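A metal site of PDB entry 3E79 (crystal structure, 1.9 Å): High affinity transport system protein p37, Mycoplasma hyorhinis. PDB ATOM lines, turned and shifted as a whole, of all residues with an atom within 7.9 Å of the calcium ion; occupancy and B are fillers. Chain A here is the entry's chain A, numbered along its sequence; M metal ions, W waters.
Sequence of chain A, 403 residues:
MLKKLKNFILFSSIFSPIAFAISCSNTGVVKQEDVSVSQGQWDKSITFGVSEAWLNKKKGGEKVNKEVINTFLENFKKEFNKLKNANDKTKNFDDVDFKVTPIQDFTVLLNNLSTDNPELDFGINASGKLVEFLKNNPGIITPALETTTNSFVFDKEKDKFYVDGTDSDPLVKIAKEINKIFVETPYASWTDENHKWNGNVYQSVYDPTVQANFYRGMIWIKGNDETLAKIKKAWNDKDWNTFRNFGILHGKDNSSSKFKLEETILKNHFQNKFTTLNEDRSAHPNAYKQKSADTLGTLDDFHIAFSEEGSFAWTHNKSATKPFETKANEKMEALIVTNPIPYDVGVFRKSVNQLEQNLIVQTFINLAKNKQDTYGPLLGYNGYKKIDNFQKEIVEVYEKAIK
The backbone NH (N) of Asp 121 sits at hydrogen-bond distance from the backbone carbonyl oxygen (O) of Thr 47 (3.1 Å). The backbone NH (N) of Asp 43 lies within hydrogen-bond range of the side-chain carboxylate (OE1) of Glu 356 (3.0 Å). OD2 of Asp 43 sits close to NH2 of Arg 349. N of Arg 349 is in hydrogen-bond range of O of Asp 121, at 3.0 Å.
The nearest printed residue that does not touch the calcium ion is Ile 46 (4.3 Å).
The backbone carbonyl oxygen (O) of Pro 118 is bound to the calcium ion (2.2 Å). Water W1 is bound to the calcium ion, 2.4 Å away. O of Ser 45 binds the calcium ion (2.4 Å). The calcium ion is bound by the side-chain carboxylate (OD2) of Asp 43, 2.4 Å away. The calcium ion is bound by OD1 of Asp 121, 2.4 Å away. The calcium ion is bound by water W2 (2.5 Å). The calcium ion is bound by OD2 of Asp 121.
Water W1 lies within hydrogen-bond range of OG1 of Thr 47 and OG of Ser 45.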
ATOM      1  N   ASP A  43      -9.291  27.020 -16.202  1.00  0.00           N
ATOM      2  CA  ASP A  43      -8.247  26.043 -16.560  1.00  0.00           C
ATOM      3  C   ASP A  43      -8.256  24.915 -15.551  1.00  0.00           C
ATOM      4  O   ASP A  43      -8.012  25.113 -14.362  1.00  0.00           O
ATOM      5  CB  ASP A  43      -6.877  26.721 -16.629  1.00  0.00           C
ATOM      6  CG  ASP A  43      -5.763  25.852 -17.191  1.00  0.00           C
ATOM      7  OD1 ASP A  43      -5.966  24.635 -17.379  1.00  0.00           O
ATOM      8  OD2 ASP A  43      -4.645  26.343 -17.460  1.00  0.00           O
ATOM      9  N   LYS A  44      -8.555  23.686 -15.994  1.00  0.00           N
ATOM     10  CA  LYS A  44      -8.727  22.635 -14.994  1.00  0.00           C
ATOM     11  C   LYS A  44      -7.384  22.041 -14.578  1.00  0.00           C
ATOM     12  O   LYS A  44      -7.320  21.129 -13.733  1.00  0.00           O
ATOM     13  CB  LYS A  44      -9.658  21.542 -15.520  1.00  0.00           C
ATOM     14  CG  LYS A  44      -9.284  21.079 -16.920  1.00  0.00           C
ATOM     15  CD  LYS A  44     -10.127  19.883 -17.353  1.00  0.00           C
ATOM     16  CE  LYS A  44      -9.296  18.818 -18.044  1.00  0.00           C
ATOM     17  NZ  LYS A  44     -10.023  18.193 -19.180  1.00  0.00           N
ATOM     18  N   SER A  45      -6.299  22.562 -15.148  1.00  0.00           N
ATOM     19  CA  SER A  45      -4.980  22.159 -14.665  1.00  0.00           C
ATOM     20  C   SER A  45      -4.133  23.372 -14.309  1.00  0.00           C
ATOM     21  O   SER A  45      -3.914  24.224 -15.174  1.00  0.00           O
ATOM     22  CB  SER A  45      -4.261  21.299 -15.708  1.00  0.00           C
ATOM     23  OG  SER A  45      -2.915  21.104 -15.318  1.00  0.00           O
ATOM     24  N   ILE A  46      -3.653  23.477 -13.067  1.00  0.00           N
ATOM     25  CA  ILE A  46      -2.910  24.672 -12.665  1.00  0.00           C
ATOM     26  C   ILE A  46      -1.495  24.281 -12.268  1.00  0.00           C
ATOM     27  O   ILE A  46      -1.307  23.482 -11.347  1.00  0.00           O
ATOM     28  CB  ILE A  46      -3.619  25.459 -11.538  1.00  0.00           C
ATOM     29  CG1 ILE A  46      -4.921  26.141 -11.988  1.00  0.00           C
ATOM     30  CG2 ILE A  46      -2.690  26.473 -10.886  1.00  0.00           C
ATOM     31  CD1 ILE A  46      -4.699  27.252 -12.994  1.00  0.00           C
ATOM     32  N   THR A  47      -0.516  24.829 -12.979  1.00  0.00           N
ATOM     33  CA  THR A  47       0.897  24.529 -12.806  1.00  0.00           C
ATOM     34  C   THR A  47       1.662  25.709 -12.213  1.00  0.00           C
ATOM     35  O   THR A  47       1.716  26.765 -12.844  1.00  0.00           O
ATOM     36  CB  THR A  47       1.536  24.144 -14.164  1.00  0.00           C
ATOM     37  OG1 THR A  47       0.933  22.922 -14.588  1.00  0.00           O
ATOM     38  CG2 THR A  47       3.032  23.866 -14.048  1.00  0.00           C
ATOM     39  N   PHE A  48       2.228  25.496 -11.024  1.00  0.00           N
ATOM     40  CA  PHE A  48       3.087  26.455 -10.344  1.00  0.00           C
ATOM     41  C   PHE A  48       4.547  26.330 -10.777  1.00  0.00           C
ATOM     42  O   PHE A  48       5.055  25.213 -10.729  1.00  0.00           O
ATOM     43  CB  PHE A  48       3.044  26.237  -8.833  1.00  0.00           C
ATOM     44  CG  PHE A  48       1.724  26.447  -8.149  1.00  0.00           C
ATOM     45  CD1 PHE A  48       0.767  27.298  -8.686  1.00  0.00           C
ATOM     46  CD2 PHE A  48       1.443  25.795  -6.960  1.00  0.00           C
ATOM     47  CE1 PHE A  48      -0.442  27.481  -8.041  1.00  0.00           C
ATOM     48  CE2 PHE A  48       0.227  25.973  -6.320  1.00  0.00           C
ATOM     49  CZ  PHE A  48      -0.716  26.816  -6.869  1.00  0.00           C
ATOM     50  N   VAL A  96     -10.220  21.283 -10.097  1.00  0.00           N
ATOM     51  CA  VAL A  96      -8.910  21.639 -10.657  1.00  0.00           C
ATOM     52  C   VAL A  96      -7.787  20.827 -10.042  1.00  0.00           C
ATOM     53  O   VAL A  96      -7.744  20.578  -8.834  1.00  0.00           O
ATOM     54  CB  VAL A  96      -8.632  23.152 -10.434  1.00  0.00           C
ATOM     55  CG1 VAL A  96      -7.279  23.558 -10.981  1.00  0.00           C
ATOM     56  CG2 VAL A  96      -9.722  23.981 -11.109  1.00  0.00           C
ATOM     57  N   ASP A  97      -6.843  20.384 -10.866  1.00  0.00           N
ATOM     58  CA  ASP A  97      -5.687  19.670 -10.338  1.00  0.00           C
ATOM     59  C   ASP A  97      -4.488  20.619 -10.314  1.00  0.00           C
ATOM     60  O   ASP A  97      -4.354  21.496 -11.178  1.00  0.00           O
ATOM     61  CB  ASP A  97      -5.395  18.434 -11.183  1.00  0.00           C
ATOM     62  CG  ASP A  97      -4.274  17.578 -10.624  1.00  0.00           C
ATOM     63  OD1 ASP A  97      -4.400  17.078  -9.490  1.00  0.00           O
ATOM     64  OD2 ASP A  97      -3.244  17.415 -11.321  1.00  0.00           O
ATOM     65  N   LYS A  99      -0.189  21.235 -10.050  1.00  0.00           N
ATOM     66  CA  LYS A  99       1.145  20.623 -10.178  1.00  0.00           C
ATOM     67  C   LYS A  99       2.226  21.693 -10.125  1.00  0.00           C
ATOM     68  O   LYS A  99       1.926  22.890 -10.094  1.00  0.00           O
ATOM     69  CB  LYS A  99       1.273  19.828 -11.476  1.00  0.00           C
ATOM     70  CG  LYS A  99       0.128  20.026 -12.454  1.00  0.00           C
ATOM     71  CD  LYS A  99       0.184  19.007 -13.582  1.00  0.00           C
ATOM     72  CE  LYS A  99      -1.212  18.595 -14.034  1.00  0.00           C
ATOM     73  NZ  LYS A  99      -1.345  17.110 -14.160  1.00  0.00           N
ATOM     74  N   ASN A 117       0.795  30.718 -21.909  1.00  0.00           N
ATOM     75  CA  ASN A 117       0.734  29.294 -22.202  1.00  0.00           C
ATOM     76  C   ASN A 117       0.176  28.517 -21.019  1.00  0.00           C
ATOM     77  O   ASN A 117       0.714  28.628 -19.902  1.00  0.00           O
ATOM     78  CB  ASN A 117       2.144  28.842 -22.566  1.00  0.00           C
ATOM     79  CG  ASN A 117       2.085  27.437 -23.144  1.00  0.00           C
ATOM     80  OD1 ASN A 117       1.422  26.569 -22.594  1.00  0.00           O
ATOM     81  ND2 ASN A 117       2.786  27.232 -24.241  1.00  0.00           N
ATOM     82  N   PRO A 118      -0.893  27.760 -21.191  1.00  0.00           N
ATOM     83  CA  PRO A 118      -1.504  26.983 -20.103  1.00  0.00           C
ATOM     84  C   PRO A 118      -0.599  25.975 -19.423  1.00  0.00           C
ATOM     85  O   PRO A 118      -0.948  25.443 -18.370  1.00  0.00           O
ATOM     86  CB  PRO A 118      -2.632  26.204 -20.821  1.00  0.00           C
ATOM     87  CG  PRO A 118      -2.990  27.121 -21.943  1.00  0.00           C
ATOM     88  CD  PRO A 118      -1.656  27.623 -22.447  1.00  0.00           C
ATOM     89  N   GLU A 119       0.563  25.662 -19.991  1.00  0.00           N
ATOM     90  CA  GLU A 119       1.477  24.758 -19.276  1.00  0.00           C
ATOM     91  C   GLU A 119       2.150  25.451 -18.100  1.00  0.00           C
ATOM     92  O   GLU A 119       2.767  24.779 -17.273  1.00  0.00           O
ATOM     93  CB  GLU A 119       2.565  24.207 -20.194  1.00  0.00           C
ATOM     94  CG  GLU A 119       3.304  25.242 -21.004  1.00  0.00           C
ATOM     95  CD  GLU A 119       4.527  25.838 -20.345  1.00  0.00           C
ATOM     96  OE1 GLU A 119       5.139  25.172 -19.478  1.00  0.00           O
ATOM     97  OE2 GLU A 119       4.904  26.979 -20.700  1.00  0.00           O
ATOM     98  N   LEU A 120       2.060  26.768 -18.003  1.00  0.00           N
ATOM     99  CA  LEU A 120       2.653  27.473 -16.859  1.00  0.00           C
ATOM    100  C   LEU A 120       1.710  28.590 -16.472  1.00  0.00           C
ATOM    101  O   LEU A 120       1.537  29.531 -17.244  1.00  0.00           O
ATOM    102  CB  LEU A 120       4.045  28.020 -17.194  1.00  0.00           C
ATOM    103  CG  LEU A 120       4.740  28.709 -16.008  1.00  0.00           C
ATOM    104  CD1 LEU A 120       4.962  27.690 -14.898  1.00  0.00           C
ATOM    105  CD2 LEU A 120       6.037  29.363 -16.431  1.00  0.00           C
ATOM    106  N   ASP A 121       1.080  28.495 -15.306  1.00  0.00           N
ATOM    107  CA  ASP A 121       0.013  29.433 -14.981  1.00  0.00           C
ATOM    108  C   ASP A 121       0.351  30.479 -13.928  1.00  0.00           C
ATOM    109  O   ASP A 121      -0.254  31.551 -13.901  1.00  0.00           O
ATOM    110  CB  ASP A 121      -1.174  28.618 -14.427  1.00  0.00           C
ATOM    111  CG  ASP A 121      -1.589  27.578 -15.470  1.00  0.00           C
ATOM    112  OD1 ASP A 121      -1.306  26.403 -15.212  1.00  0.00           O
ATOM    113  OD2 ASP A 121      -2.029  28.011 -16.560  1.00  0.00           O
ATOM    114  N   PHE A 122       1.278  30.172 -13.034  1.00  0.00           N
ATOM    115  CA  PHE A 122       1.449  31.044 -11.874  1.00  0.00           C
ATOM    116  C   PHE A 122       2.852  30.877 -11.320  1.00  0.00           C
ATOM    117  O   PHE A 122       3.382  29.768 -11.440  1.00  0.00           O
ATOM    118  CB  PHE A 122       0.408  30.664 -10.833  1.00  0.00           C
ATOM    119  CG  PHE A 122       0.543  31.293  -9.463  1.00  0.00           C
ATOM    120  CD1 PHE A 122      -0.065  32.499  -9.199  1.00  0.00           C
ATOM    121  CD2 PHE A 122       1.268  30.678  -8.453  1.00  0.00           C
ATOM    122  CE1 PHE A 122       0.072  33.109  -7.967  1.00  0.00           C
ATOM    123  CE2 PHE A 122       1.418  31.280  -7.215  1.00  0.00           C
ATOM    124  CZ  PHE A 122       0.788  32.482  -6.973  1.00  0.00           C
ATOM    125  N   ARG A 349      -0.468  34.118 -15.467  1.00  0.00           N
ATOM    126  CA  ARG A 349      -0.598  34.401 -16.904  1.00  0.00           C
ATOM    127  C   ARG A 349      -1.960  35.063 -17.102  1.00  0.00           C
ATOM    128  O   ARG A 349      -2.860  34.938 -16.275  1.00  0.00           O
ATOM    129  CB  ARG A 349      -0.449  33.157 -17.771  1.00  0.00           C
ATOM    130  CG  ARG A 349      -1.554  32.136 -17.581  1.00  0.00           C
ATOM    131  CD  ARG A 349      -1.416  30.980 -18.562  1.00  0.00           C
ATOM    132  NE  ARG A 349      -2.309  29.863 -18.209  1.00  0.00           N
ATOM    133  CZ  ARG A 349      -3.491  29.788 -18.837  1.00  0.00           C
ATOM    134  NH1 ARG A 349      -3.761  30.736 -19.727  1.00  0.00           N
ATOM    135  NH2 ARG A 349      -4.338  28.816 -18.592  1.00  0.00           N
ATOM    136  N   VAL A 352      -5.900  33.289 -17.170  1.00  0.00           N
ATOM    137  CA  VAL A 352      -6.566  32.413 -16.191  1.00  0.00           C
ATOM    138  C   VAL A 352      -7.821  33.135 -15.731  1.00  0.00           C
ATOM    139  O   VAL A 352      -7.755  34.326 -15.426  1.00  0.00           O
ATOM    140  CB  VAL A 352      -5.662  32.067 -15.004  1.00  0.00           C
ATOM    141  CG1 VAL A 352      -6.401  31.275 -13.916  1.00  0.00           C
ATOM    142  CG2 VAL A 352      -4.459  31.282 -15.511  1.00  0.00           C
ATOM    143  N   GLU A 356     -11.199  31.987 -10.918  1.00  0.00           N
ATOM    144  CA  GLU A 356     -10.221  30.974 -10.525  1.00  0.00           C
ATOM    145  C   GLU A 356      -9.037  31.582  -9.766  1.00  0.00           C
ATOM    146  O   GLU A 356      -8.588  31.030  -8.764  1.00  0.00           O
ATOM    147  CB  GLU A 356      -9.702  30.215 -11.772  1.00  0.00           C
ATOM    148  CG  GLU A 356      -9.032  28.896 -11.403  1.00  0.00           C
ATOM    149  CD  GLU A 356      -8.674  28.063 -12.611  1.00  0.00           C
ATOM    150  OE1 GLU A 356      -8.760  28.606 -13.732  1.00  0.00           O
ATOM    151  OE2 GLU A 356      -8.302  26.888 -12.421  1.00  0.00           O
HETATM  152 CA    CA M   1      -2.579  25.218 -16.917  1.00  0.00          CA
HETATM  153  O   HOH W   1      -1.188  23.368 -16.438  1.00  0.00           O
HETATM  154  O   HOH W   2      -3.728  23.701 -18.467  1.00  0.00           O
